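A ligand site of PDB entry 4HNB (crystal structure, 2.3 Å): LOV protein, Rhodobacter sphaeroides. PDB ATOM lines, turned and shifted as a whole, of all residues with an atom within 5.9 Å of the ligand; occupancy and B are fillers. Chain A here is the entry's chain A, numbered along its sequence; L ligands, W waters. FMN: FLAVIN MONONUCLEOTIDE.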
ATOM      1  N   THR A  22     -10.922  11.934   6.619  1.00  0.00           N
ATOM      2  CA  THR A  22      -9.573  12.124   7.126  1.00  0.00           C
ATOM      3  C   THR A  22      -9.621  13.179   8.230  1.00  0.00           C
ATOM      4  O   THR A  22     -10.406  14.131   8.158  1.00  0.00           O
ATOM      5  CB  THR A  22      -8.598  12.585   6.037  1.00  0.00           C
ATOM      6  OG1 THR A  22      -9.257  13.489   5.146  1.00  0.00           O
ATOM      7  CG2 THR A  22      -8.068  11.407   5.237  1.00  0.00           C
ATOM      8  N   LEU A  23      -8.789  13.016   9.261  1.00  0.00           N
ATOM      9  CA  LEU A  23      -8.682  14.035  10.302  1.00  0.00           C
ATOM     10  C   LEU A  23      -7.218  14.444  10.460  1.00  0.00           C
ATOM     11  O   LEU A  23      -6.346  13.596  10.665  1.00  0.00           O
ATOM     12  CB  LEU A  23      -9.255  13.541  11.629  1.00  0.00           C
ATOM     13  CG  LEU A  23      -9.655  14.616  12.647  1.00  0.00           C
ATOM     14  CD1 LEU A  23     -11.037  15.162  12.316  1.00  0.00           C
ATOM     15  CD2 LEU A  23      -9.618  14.095  14.068  1.00  0.00           C
ATOM     16  N   VAL A  24      -6.967  15.746  10.360  1.00  0.00           N
ATOM     17  CA  VAL A  24      -5.611  16.275  10.531  1.00  0.00           C
ATOM     18  C   VAL A  24      -5.477  17.020  11.869  1.00  0.00           C
ATOM     19  O   VAL A  24      -6.402  17.718  12.296  1.00  0.00           O
ATOM     20  CB  VAL A  24      -5.223  17.168   9.336  1.00  0.00           C
ATOM     21  CG1 VAL A  24      -4.097  18.119   9.710  1.00  0.00           C
ATOM     22  CG2 VAL A  24      -4.831  16.305   8.140  1.00  0.00           C
ATOM     23  N   MET A  26      -4.056  19.928  13.978  1.00  0.00           N
ATOM     24  CA  MET A  26      -3.603  21.292  13.717  1.00  0.00           C
ATOM     25  C   MET A  26      -2.488  21.701  14.685  1.00  0.00           C
ATOM     26  O   MET A  26      -1.809  22.699  14.465  1.00  0.00           O
ATOM     27  CB  MET A  26      -4.762  22.286  13.814  1.00  0.00           C
ATOM     28  CG  MET A  26      -5.851  22.111  12.768  1.00  0.00           C
ATOM     29  SD  MET A  26      -5.233  21.965  11.078  1.00  0.00           S
ATOM     30  CE  MET A  26      -5.108  23.677  10.577  1.00  0.00           C
ATOM     31  N   GLN A  31       1.334  19.331  10.263  1.00  0.00           N
ATOM     32  CA  GLN A  31      -0.111  19.086  10.111  1.00  0.00           C
ATOM     33  C   GLN A  31      -0.425  17.700   9.565  1.00  0.00           C
ATOM     34  O   GLN A  31      -0.811  17.551   8.407  1.00  0.00           O
ATOM     35  CB  GLN A  31      -0.776  20.163   9.245  1.00  0.00           C
ATOM     36  CG  GLN A  31      -0.824  21.537   9.893  1.00  0.00           C
ATOM     37  CD  GLN A  31      -1.472  22.588   9.007  1.00  0.00           C
ATOM     38  OE1 GLN A  31      -1.497  22.438   7.787  1.00  0.00           O
ATOM     39  NE2 GLN A  31      -1.997  23.639   9.611  1.00  0.00           N
ATOM     40  N   LEU A  33      -1.811  13.627   9.196  1.00  0.00           N
ATOM     41  CA  LEU A  33      -2.922  12.704   9.332  1.00  0.00           C
ATOM     42  C   LEU A  33      -2.938  12.077  10.717  1.00  0.00           C
ATOM     43  O   LEU A  33      -1.932  11.564  11.193  1.00  0.00           O
ATOM     44  CB  LEU A  33      -2.827  11.604   8.281  1.00  0.00           C
ATOM     45  CG  LEU A  33      -3.378  11.994   6.917  1.00  0.00           C
ATOM     46  CD1 LEU A  33      -3.057  10.918   5.901  1.00  0.00           C
ATOM     47  CD2 LEU A  33      -4.875  12.237   7.015  1.00  0.00           C
ATOM     48  N   PHE A  40     -11.295   5.943   2.451  1.00  0.00           N
ATOM     49  CA  PHE A  40     -10.139   6.721   2.029  1.00  0.00           C
ATOM     50  C   PHE A  40      -8.984   5.799   1.598  1.00  0.00           C
ATOM     51  O   PHE A  40      -8.407   5.945   0.518  1.00  0.00           O
ATOM     52  CB  PHE A  40      -9.674   7.663   3.142  1.00  0.00           C
ATOM     53  CG  PHE A  40      -8.380   8.343   2.831  1.00  0.00           C
ATOM     54  CD1 PHE A  40      -8.337   9.405   1.939  1.00  0.00           C
ATOM     55  CD2 PHE A  40      -7.188   7.898   3.406  1.00  0.00           C
ATOM     56  CE1 PHE A  40      -7.121  10.019   1.637  1.00  0.00           C
ATOM     57  CE2 PHE A  40      -5.978   8.512   3.116  1.00  0.00           C
ATOM     58  CZ  PHE A  40      -5.939   9.566   2.223  1.00  0.00           C
ATOM     59  N   ASN A  55       1.657  14.358   6.457  1.00  0.00           N
ATOM     60  CA  ASN A  55       0.729  15.345   5.893  1.00  0.00           C
ATOM     61  C   ASN A  55       0.139  14.838   4.574  1.00  0.00           C
ATOM     62  O   ASN A  55       0.855  14.176   3.813  1.00  0.00           O
ATOM     63  CB  ASN A  55       1.455  16.682   5.664  1.00  0.00           C
ATOM     64  CG  ASN A  55       0.508  17.813   5.272  1.00  0.00           C
ATOM     65  OD1 ASN A  55       0.293  18.085   4.085  1.00  0.00           O
ATOM     66  ND2 ASN A  55      -0.046  18.498   6.267  1.00  0.00           N
ATOM     67  N   CYS A  56      -1.129  15.148   4.302  1.00  0.00           N
ATOM     68  CA  CYS A  56      -1.822  14.640   3.108  1.00  0.00           C
ATOM     69  C   CYS A  56      -1.237  15.095   1.790  1.00  0.00           C
ATOM     70  O   CYS A  56      -1.666  14.629   0.751  1.00  0.00           O
ATOM     71  CB  CYS A  56      -3.314  15.009   3.091  1.00  0.00           C
ATOM     72  SG  CYS A  56      -4.222  14.544   4.553  1.00  0.00           S
ATOM     73  N   ARG A  57      -0.272  16.010   1.822  1.00  0.00           N
ATOM     74  CA  ARG A  57       0.296  16.489   0.556  1.00  0.00           C
ATOM     75  C   ARG A  57       1.122  15.416  -0.223  1.00  0.00           C
ATOM     76  O   ARG A  57       1.578  15.669  -1.343  1.00  0.00           O
ATOM     77  CB  ARG A  57       1.033  17.829   0.759  1.00  0.00           C
ATOM     78  CG  ARG A  57       2.563  17.761   1.004  1.00  0.00           C
ATOM     79  CD  ARG A  57       3.123  19.089   1.574  1.00  0.00           C
ATOM     80  NE  ARG A  57       3.429  18.977   3.000  1.00  0.00           N
ATOM     81  CZ  ARG A  57       2.966  19.770   3.948  1.00  0.00           C
ATOM     82  NH1 ARG A  57       3.303  19.561   5.218  1.00  0.00           N
ATOM     83  NH2 ARG A  57       2.166  20.780   3.648  1.00  0.00           N
ATOM     84  N   LEU A  59      -0.182  12.884  -1.560  1.00  0.00           N
ATOM     85  CA  LEU A  59      -1.070  12.456  -2.629  1.00  0.00           C
ATOM     86  C   LEU A  59      -0.791  13.248  -3.897  1.00  0.00           C
ATOM     87  O   LEU A  59      -1.176  12.833  -4.992  1.00  0.00           O
ATOM     88  CB  LEU A  59      -2.537  12.593  -2.180  1.00  0.00           C
ATOM     89  CG  LEU A  59      -2.974  11.588  -1.099  1.00  0.00           C
ATOM     90  CD1 LEU A  59      -4.159  12.078  -0.268  1.00  0.00           C
ATOM     91  CD2 LEU A  59      -3.307  10.283  -1.750  1.00  0.00           C
ATOM     92  N   GLN A  60      -0.090  14.368  -3.749  1.00  0.00           N
ATOM     93  CA  GLN A  60       0.249  15.222  -4.884  1.00  0.00           C
ATOM     94  C   GLN A  60       1.666  14.954  -5.335  1.00  0.00           C
ATOM     95  O   GLN A  60       2.425  14.264  -4.642  1.00  0.00           O
ATOM     96  CB  GLN A  60       0.122  16.704  -4.500  1.00  0.00           C
ATOM     97  CG  GLN A  60      -1.142  17.056  -3.716  1.00  0.00           C
ATOM     98  CD  GLN A  60      -1.033  18.407  -3.045  1.00  0.00           C
ATOM     99  OE1 GLN A  60      -0.365  19.304  -3.567  1.00  0.00           O
ATOM    100  NE2 GLN A  60      -1.672  18.561  -1.887  1.00  0.00           N
ATOM    101  N   ASN A  65      -0.686  21.780  -7.738  1.00  0.00           N
ATOM    102  CA  ASN A  65      -1.862  22.380  -7.122  1.00  0.00           C
ATOM    103  C   ASN A  65      -1.521  23.686  -6.388  1.00  0.00           C
ATOM    104  O   ASN A  65      -1.997  23.897  -5.276  1.00  0.00           O
ATOM    105  CB  ASN A  65      -2.504  21.402  -6.136  1.00  0.00           C
ATOM    106  CG  ASN A  65      -2.735  20.019  -6.736  1.00  0.00           C
ATOM    107  OD1 ASN A  65      -3.366  19.863  -7.783  1.00  0.00           O
ATOM    108  ND2 ASN A  65      -2.209  18.991  -6.054  1.00  0.00           N
ATOM    109  N   ARG A  69      -3.685  24.816  -3.230  1.00  0.00           N
ATOM    110  CA  ARG A  69      -3.039  24.727  -1.919  1.00  0.00           C
ATOM    111  C   ARG A  69      -2.981  26.088  -1.241  1.00  0.00           C
ATOM    112  O   ARG A  69      -2.997  26.177  -0.011  1.00  0.00           O
ATOM    113  CB  ARG A  69      -1.627  24.140  -2.019  1.00  0.00           C
ATOM    114  CG  ARG A  69      -1.555  22.638  -2.285  1.00  0.00           C
ATOM    115  CD  ARG A  69      -0.132  22.140  -2.074  1.00  0.00           C
ATOM    116  NE  ARG A  69       0.858  23.185  -2.299  1.00  0.00           N
ATOM    117  CZ  ARG A  69       1.386  23.458  -3.488  1.00  0.00           C
ATOM    118  NH1 ARG A  69       2.283  24.424  -3.607  1.00  0.00           N
ATOM    119  NH2 ARG A  69       1.035  22.746  -4.556  1.00  0.00           N
ATOM    120  N   ALA A  70      -2.903  27.150  -2.037  1.00  0.00           N
ATOM    121  CA  ALA A  70      -3.025  28.498  -1.501  1.00  0.00           C
ATOM    122  C   ALA A  70      -4.406  28.649  -0.861  1.00  0.00           C
ATOM    123  O   ALA A  70      -4.515  29.042   0.297  1.00  0.00           O
ATOM    124  CB  ALA A  70      -2.811  29.539  -2.584  1.00  0.00           C
ATOM    125  N   ILE A  72      -6.221  26.294   0.157  1.00  0.00           N
ATOM    126  CA  ILE A  72      -6.280  25.390   1.307  1.00  0.00           C
ATOM    127  C   ILE A  72      -5.626  25.997   2.543  1.00  0.00           C
ATOM    128  O   ILE A  72      -6.209  25.971   3.638  1.00  0.00           O
ATOM    129  CB  ILE A  72      -5.706  23.993   0.980  1.00  0.00           C
ATOM    130  CG1 ILE A  72      -6.655  23.243   0.045  1.00  0.00           C
ATOM    131  CG2 ILE A  72      -5.519  23.195   2.262  1.00  0.00           C
ATOM    132  CD1 ILE A  72      -6.047  22.048  -0.675  1.00  0.00           C
ATOM    133  N   ARG A  73      -4.438  26.580   2.349  1.00  0.00           N
ATOM    134  CA  ARG A  73      -3.706  27.221   3.452  1.00  0.00           C
ATOM    135  C   ARG A  73      -4.485  28.385   4.078  1.00  0.00           C
ATOM    136  O   ARG A  73      -4.556  28.507   5.309  1.00  0.00           O
ATOM    137  CB  ARG A  73      -2.301  27.630   2.981  1.00  0.00           C
ATOM    138  CG  ARG A  73      -1.379  26.426   2.667  1.00  0.00           C
ATOM    139  CD  ARG A  73       0.079  26.813   2.334  1.00  0.00           C
ATOM    140  NE  ARG A  73       0.173  27.844   1.305  1.00  0.00           N
ATOM    141  CZ  ARG A  73       0.321  27.599   0.006  1.00  0.00           C
ATOM    142  NH1 ARG A  73       0.404  26.356  -0.435  1.00  0.00           N
ATOM    143  NH2 ARG A  73       0.380  28.608  -0.849  1.00  0.00           N
ATOM    144  N   LEU A  76      -7.338  26.888   6.105  1.00  0.00           N
ATOM    145  CA  LEU A  76      -6.850  26.253   7.332  1.00  0.00           C
ATOM    146  C   LEU A  76      -6.460  27.297   8.381  1.00  0.00           C
ATOM    147  O   LEU A  76      -6.763  27.150   9.563  1.00  0.00           O
ATOM    148  CB  LEU A  76      -5.674  25.312   7.040  1.00  0.00           C
ATOM    149  CG  LEU A  76      -5.927  24.142   6.064  1.00  0.00           C
ATOM    150  CD1 LEU A  76      -4.662  23.304   5.787  1.00  0.00           C
ATOM    151  CD2 LEU A  76      -7.072  23.280   6.540  1.00  0.00           C
ATOM    152  N   LEU A  86      -8.252  18.693  -6.133  1.00  0.00           N
ATOM    153  CA  LEU A  86      -6.816  18.440  -6.204  1.00  0.00           C
ATOM    154  C   LEU A  86      -6.497  17.310  -7.199  1.00  0.00           C
ATOM    155  O   LEU A  86      -7.235  16.316  -7.269  1.00  0.00           O
ATOM    156  CB  LEU A  86      -6.286  18.057  -4.812  1.00  0.00           C
ATOM    157  CG  LEU A  86      -6.355  19.156  -3.747  1.00  0.00           C
ATOM    158  CD1 LEU A  86      -6.009  18.662  -2.345  1.00  0.00           C
ATOM    159  CD2 LEU A  86      -5.441  20.313  -4.172  1.00  0.00           C
ATOM    160  N   ARG A  87      -5.428  17.468  -7.963  1.00  0.00           N
ATOM    161  CA  ARG A  87      -4.890  16.350  -8.743  1.00  0.00           C
ATOM    162  C   ARG A  87      -4.210  15.420  -7.767  1.00  0.00           C
ATOM    163  O   ARG A  87      -3.410  15.862  -6.956  1.00  0.00           O
ATOM    164  CB  ARG A  87      -3.882  16.827  -9.786  1.00  0.00           C
ATOM    165  CG  ARG A  87      -3.010  15.731 -10.382  1.00  0.00           C
ATOM    166  CD  ARG A  87      -3.810  14.775 -11.253  1.00  0.00           C
ATOM    167  NE  ARG A  87      -4.536  15.502 -12.298  1.00  0.00           N
ATOM    168  CZ  ARG A  87      -5.109  14.933 -13.348  1.00  0.00           C
ATOM    169  NH1 ARG A  87      -5.045  13.622 -13.521  1.00  0.00           N
ATOM    170  NH2 ARG A  87      -5.738  15.685 -14.246  1.00  0.00           N
ATOM    171  N   ASN A  88      -4.521  14.133  -7.818  1.00  0.00           N
ATOM    172  CA  ASN A  88      -3.931  13.207  -6.847  1.00  0.00           C
ATOM    173  C   ASN A  88      -3.430  11.895  -7.464  1.00  0.00           C
ATOM    174  O   ASN A  88      -3.653  11.628  -8.640  1.00  0.00           O
ATOM    175  CB  ASN A  88      -4.876  12.953  -5.672  1.00  0.00           C
ATOM    176  CG  ASN A  88      -4.726  13.992  -4.566  1.00  0.00           C
ATOM    177  OD1 ASN A  88      -5.447  13.965  -3.569  1.00  0.00           O
ATOM    178  ND2 ASN A  88      -3.778  14.910  -4.741  1.00  0.00           N
ATOM    179  N   ASN A  98      -9.321  14.732  -7.175  1.00  0.00           N
ATOM    180  CA  ASN A  98      -9.924  14.653  -5.862  1.00  0.00           C
ATOM    181  C   ASN A  98     -10.734  15.916  -5.642  1.00  0.00           C
ATOM    182  O   ASN A  98     -10.189  17.008  -5.677  1.00  0.00           O
ATOM    183  CB  ASN A  98      -8.779  14.580  -4.839  1.00  0.00           C
ATOM    184  CG  ASN A  98      -9.235  14.281  -3.422  1.00  0.00           C
ATOM    185  OD1 ASN A  98      -8.452  13.767  -2.627  1.00  0.00           O
ATOM    186  ND2 ASN A  98     -10.479  14.607  -3.084  1.00  0.00           N
ATOM    187  N   LEU A 100     -12.065  17.701  -2.859  1.00  0.00           N
ATOM    188  CA  LEU A 100     -11.791  17.645  -1.424  1.00  0.00           C
ATOM    189  C   LEU A 100     -12.676  18.612  -0.637  1.00  0.00           C
ATOM    190  O   LEU A 100     -12.775  19.805  -0.965  1.00  0.00           O
ATOM    191  CB  LEU A 100     -10.296  17.927  -1.173  1.00  0.00           C
ATOM    192  CG  LEU A 100      -9.844  18.057   0.280  1.00  0.00           C
ATOM    193  CD1 LEU A 100      -9.816  16.710   0.979  1.00  0.00           C
ATOM    194  CD2 LEU A 100      -8.486  18.752   0.377  1.00  0.00           C
ATOM    195  N   LEU A 102     -13.242  20.376   2.970  1.00  0.00           N
ATOM    196  CA  LEU A 102     -12.559  20.709   4.228  1.00  0.00           C
ATOM    197  C   LEU A 102     -13.487  21.303   5.281  1.00  0.00           C
ATOM    198  O   LEU A 102     -14.268  22.219   4.978  1.00  0.00           O
ATOM    199  CB  LEU A 102     -11.402  21.689   3.973  1.00  0.00           C
ATOM    200  CG  LEU A 102      -9.970  21.200   3.760  1.00  0.00           C
ATOM    201  CD1 LEU A 102      -9.887  19.696   3.872  1.00  0.00           C
ATOM    202  CD2 LEU A 102      -9.419  21.682   2.416  1.00  0.00           C
ATOM    203  N   PHE A 115      -8.872  19.620  11.383  1.00  0.00           N
ATOM    204  CA  PHE A 115      -9.599  19.725  10.141  1.00  0.00           C
ATOM    205  C   PHE A 115     -10.030  18.335   9.681  1.00  0.00           C
ATOM    206  O   PHE A 115      -9.284  17.363   9.792  1.00  0.00           O
ATOM    207  CB  PHE A 115      -8.768  20.438   9.079  1.00  0.00           C
ATOM    208  CG  PHE A 115      -9.222  21.845   8.822  1.00  0.00           C
ATOM    209  CD1 PHE A 115     -10.177  22.107   7.846  1.00  0.00           C
ATOM    210  CD2 PHE A 115      -8.714  22.898   9.564  1.00  0.00           C
ATOM    211  CE1 PHE A 115     -10.602  23.393   7.610  1.00  0.00           C
ATOM    212  CE2 PHE A 115      -9.142  24.195   9.341  1.00  0.00           C
ATOM    213  CZ  PHE A 115     -10.083  24.441   8.358  1.00  0.00           C
ATOM    214  N   LEU A 116     -11.274  18.262   9.219  1.00  0.00           N
ATOM    215  CA  LEU A 116     -11.853  17.049   8.667  1.00  0.00           C
ATOM    216  C   LEU A 116     -11.751  17.206   7.165  1.00  0.00           C
ATOM    217  O   LEU A 116     -12.179  18.215   6.620  1.00  0.00           O
ATOM    218  CB  LEU A 116     -13.310  16.965   9.123  1.00  0.00           C
ATOM    219  CG  LEU A 116     -14.490  16.075   8.661  1.00  0.00           C
ATOM    220  CD1 LEU A 116     -14.396  15.524   7.253  1.00  0.00           C
ATOM    221  CD2 LEU A 116     -14.831  14.984   9.665  1.00  0.00           C
ATOM    222  N   GLY A 117     -11.172  16.225   6.485  1.00  0.00           N
ATOM    223  CA  GLY A 117     -11.162  16.232   5.043  1.00  0.00           C
ATOM    224  C   GLY A 117     -11.991  15.074   4.521  1.00  0.00           C
ATOM    225  O   GLY A 117     -11.949  13.982   5.086  1.00  0.00           O
ATOM    226  N   SER A 118     -12.753  15.309   3.452  1.00  0.00           N
ATOM    227  CA  SER A 118     -13.544  14.252   2.834  1.00  0.00           C
ATOM    228  C   SER A 118     -13.331  14.256   1.333  1.00  0.00           C
ATOM    229  O   SER A 118     -13.653  15.234   0.645  1.00  0.00           O
ATOM    230  CB  SER A 118     -15.036  14.430   3.172  1.00  0.00           C
ATOM    231  OG  SER A 118     -15.780  13.320   2.710  1.00  0.00           O
ATOM    232  N   GLN A 119     -12.777  13.176   0.810  1.00  0.00           N
ATOM    233  CA  GLN A 119     -12.373  13.137  -0.586  1.00  0.00           C
ATOM    234  C   GLN A 119     -13.425  12.467  -1.454  1.00  0.00           C
ATOM    235  O   GLN A 119     -13.916  11.404  -1.111  1.00  0.00           O
ATOM    236  CB  GLN A 119     -11.026  12.396  -0.739  1.00  0.00           C
ATOM    237  CG  GLN A 119      -9.846  13.064  -0.077  1.00  0.00           C
ATOM    238  CD  GLN A 119      -9.792  12.843   1.421  1.00  0.00           C
ATOM    239  OE1 GLN A 119     -10.648  12.169   1.999  1.00  0.00           O
ATOM    240  NE2 GLN A 119      -8.796  13.436   2.057  1.00  0.00           N
HETATM  241  N1  FMN L   1      -4.221  17.100  -0.088  1.00  0.00           N
HETATM  242  C2  FMN L   1      -4.386  16.156  -1.086  1.00  0.00           C
HETATM  243  O2  FMN L   1      -3.729  16.213  -2.133  1.00  0.00           O
HETATM  244  N3  FMN L   1      -5.320  15.139  -0.956  1.00  0.00           N
HETATM  245  C4  FMN L   1      -6.053  15.071   0.205  1.00  0.00           C
HETATM  246  O4  FMN L   1      -6.881  14.173   0.349  1.00  0.00           O
HETATM  247  C4A FMN L   1      -5.895  16.006   1.225  1.00  0.00           C
HETATM  248  N5  FMN L   1      -6.661  15.899   2.367  1.00  0.00           N
HETATM  249  C5A FMN L   1      -6.510  16.815   3.386  1.00  0.00           C
HETATM  250  C6  FMN L   1      -7.282  16.676   4.544  1.00  0.00           C
HETATM  251  C7  FMN L   1      -7.141  17.596   5.566  1.00  0.00           C
HETATM  252  C7M FMN L   1      -7.981  17.447   6.795  1.00  0.00           C
HETATM  253  C8  FMN L   1      -6.221  18.629   5.443  1.00  0.00           C
HETATM  254  C8M FMN L   1      -6.072  19.624   6.562  1.00  0.00           C
HETATM  255  C9  FMN L   1      -5.455  18.769   4.297  1.00  0.00           C
HETATM  256  C9A FMN L   1      -5.578  17.854   3.260  1.00  0.00           C
HETATM  257  N10 FMN L   1      -4.801  17.947   2.102  1.00  0.00           N
HETATM  258  C10 FMN L   1      -4.966  17.027   1.076  1.00  0.00           C
HETATM  259  C1' FMN L   1      -3.836  19.075   1.911  1.00  0.00           C
HETATM  260  C2' FMN L   1      -2.472  19.050   2.583  1.00  0.00           C
HETATM  261  O2' FMN L   1      -2.555  18.438   3.863  1.00  0.00           O
HETATM  262  C3' FMN L   1      -2.024  20.506   2.681  1.00  0.00           C
HETATM  263  O3' FMN L   1      -2.817  21.160   3.643  1.00  0.00           O
HETATM  264  C4' FMN L   1      -2.177  21.270   1.372  1.00  0.00           C
HETATM  265  O4' FMN L   1      -1.522  20.547   0.351  1.00  0.00           O
HETATM  266  C5' FMN L   1      -1.578  22.687   1.460  1.00  0.00           C
HETATM  267  O5' FMN L   1      -0.332  22.582   2.109  1.00  0.00           O
HETATM  268  P   FMN L   1       1.090  22.895   1.412  1.00  0.00           P
HETATM  269  O1P FMN L   1       1.942  23.352   2.571  1.00  0.00           O
HETATM  270  O2P FMN L   1       1.652  21.659   0.761  1.00  0.00           O
HETATM  271  O3P FMN L   1       1.004  23.929   0.318  1.00  0.00           O
HETATM  272  O   HOH W   1      -2.211  20.609   6.039  1.00  0.00           O
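The side-chain sulfur (SG) of Cys 56 sits close to a nitrogen (N5) of the ligand, 3.5 Å away. The side-chain amide oxygen (OD1) of Asn 55 sits at hydrogen-bond distance from an oxygen (O2') of the ligand (2.9 Å). OD1 of Asn 88 lies within hydrogen-bond range of N3 of the ligand (2.9 Å). The side-chain amide nitrogen (NE2) of Gln 119 is in hydrogen-bond range of an oxygen (O4) of the ligand. OD1 of Asn 98 lies close to O4 of the ligand (3.4 Å). O3P of the ligand is in salt-bridge range of NE of Arg 69, at 2.7 Å. An oxygen (O4') of the ligand sits at hydrogen-bond distance from the side-chain amide nitrogen (NE2) of Gln 60 (3.0 Å). NH1 of Arg 73 lies within salt-bridge range of O3P of the ligand (2.6 Å). O1P of the ligand is in salt-bridge range of NH2 of Arg 57, 2.8 Å away.
The side-chain amide oxygen of Asn 88 sits close to the side-chain amide oxygen of Asn 98, 3.2 Å away. The side-chain amide nitrogen (ND2) of Asn 98 lies close to the backbone NH (N) of Leu 100 (3.5 Å). The backbone carbonyl oxygen (O) of Phe 115 is in hydrogen-bond range of the backbone NH (N) of Val 24 (2.9 Å). ND2 of Asn 88 sits at hydrogen-bond distance from O of Leu 59 (3.3 Å). OD1 of Asn 55 sits close to N of Arg 57, 3.1 Å away. The side-chain amide nitrogen of Asn 55 lies within hydrogen-bond range of the backbone carbonyl oxygen of Gln 31 (2.5 Å). The backbone carbonyl oxygen (O) of Arg 69 lies close to the guanidinium group (NH1) of Arg 73 (3.4 Å). The backbone carbonyl oxygen of Asn 65 lies close to the guanidinium group of Arg 69, at 3.3 Å.
OG1 of Thr 22 touches C6 of the ligand, at 3.8 Å. Val 24 touches the ligand. CD1 of Leu 59 touches N3 of the ligand, 3.3 Å away. Ile 72 touches the ligand (CG2 to O3', 3.7 Å). Leu 76 touches the ligand. Leu 86 touches the ligand. CD1 of Leu 100 touches N5 of the ligand (3.5 Å). Leu 102 touches the ligand (CD1 to C7, 3.8 Å). Phe 115 touches the ligand. Leu 116 touches the ligand (C to C7M, 3.8 Å). N of Gly 117 touches C7M of the ligand, 3.4 Å away. Along chain A the residues within 4 Å of the ligand span positions 22 to 119.
Water W1 lies within hydrogen-bond range of an oxygen (O3') of the ligand (2.5 Å), the side-chain amide oxygen (OE1) of Gln 31 (2.6 Å) and the side-chain amide nitrogen (ND2) of Asn 55 (3.0 Å).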
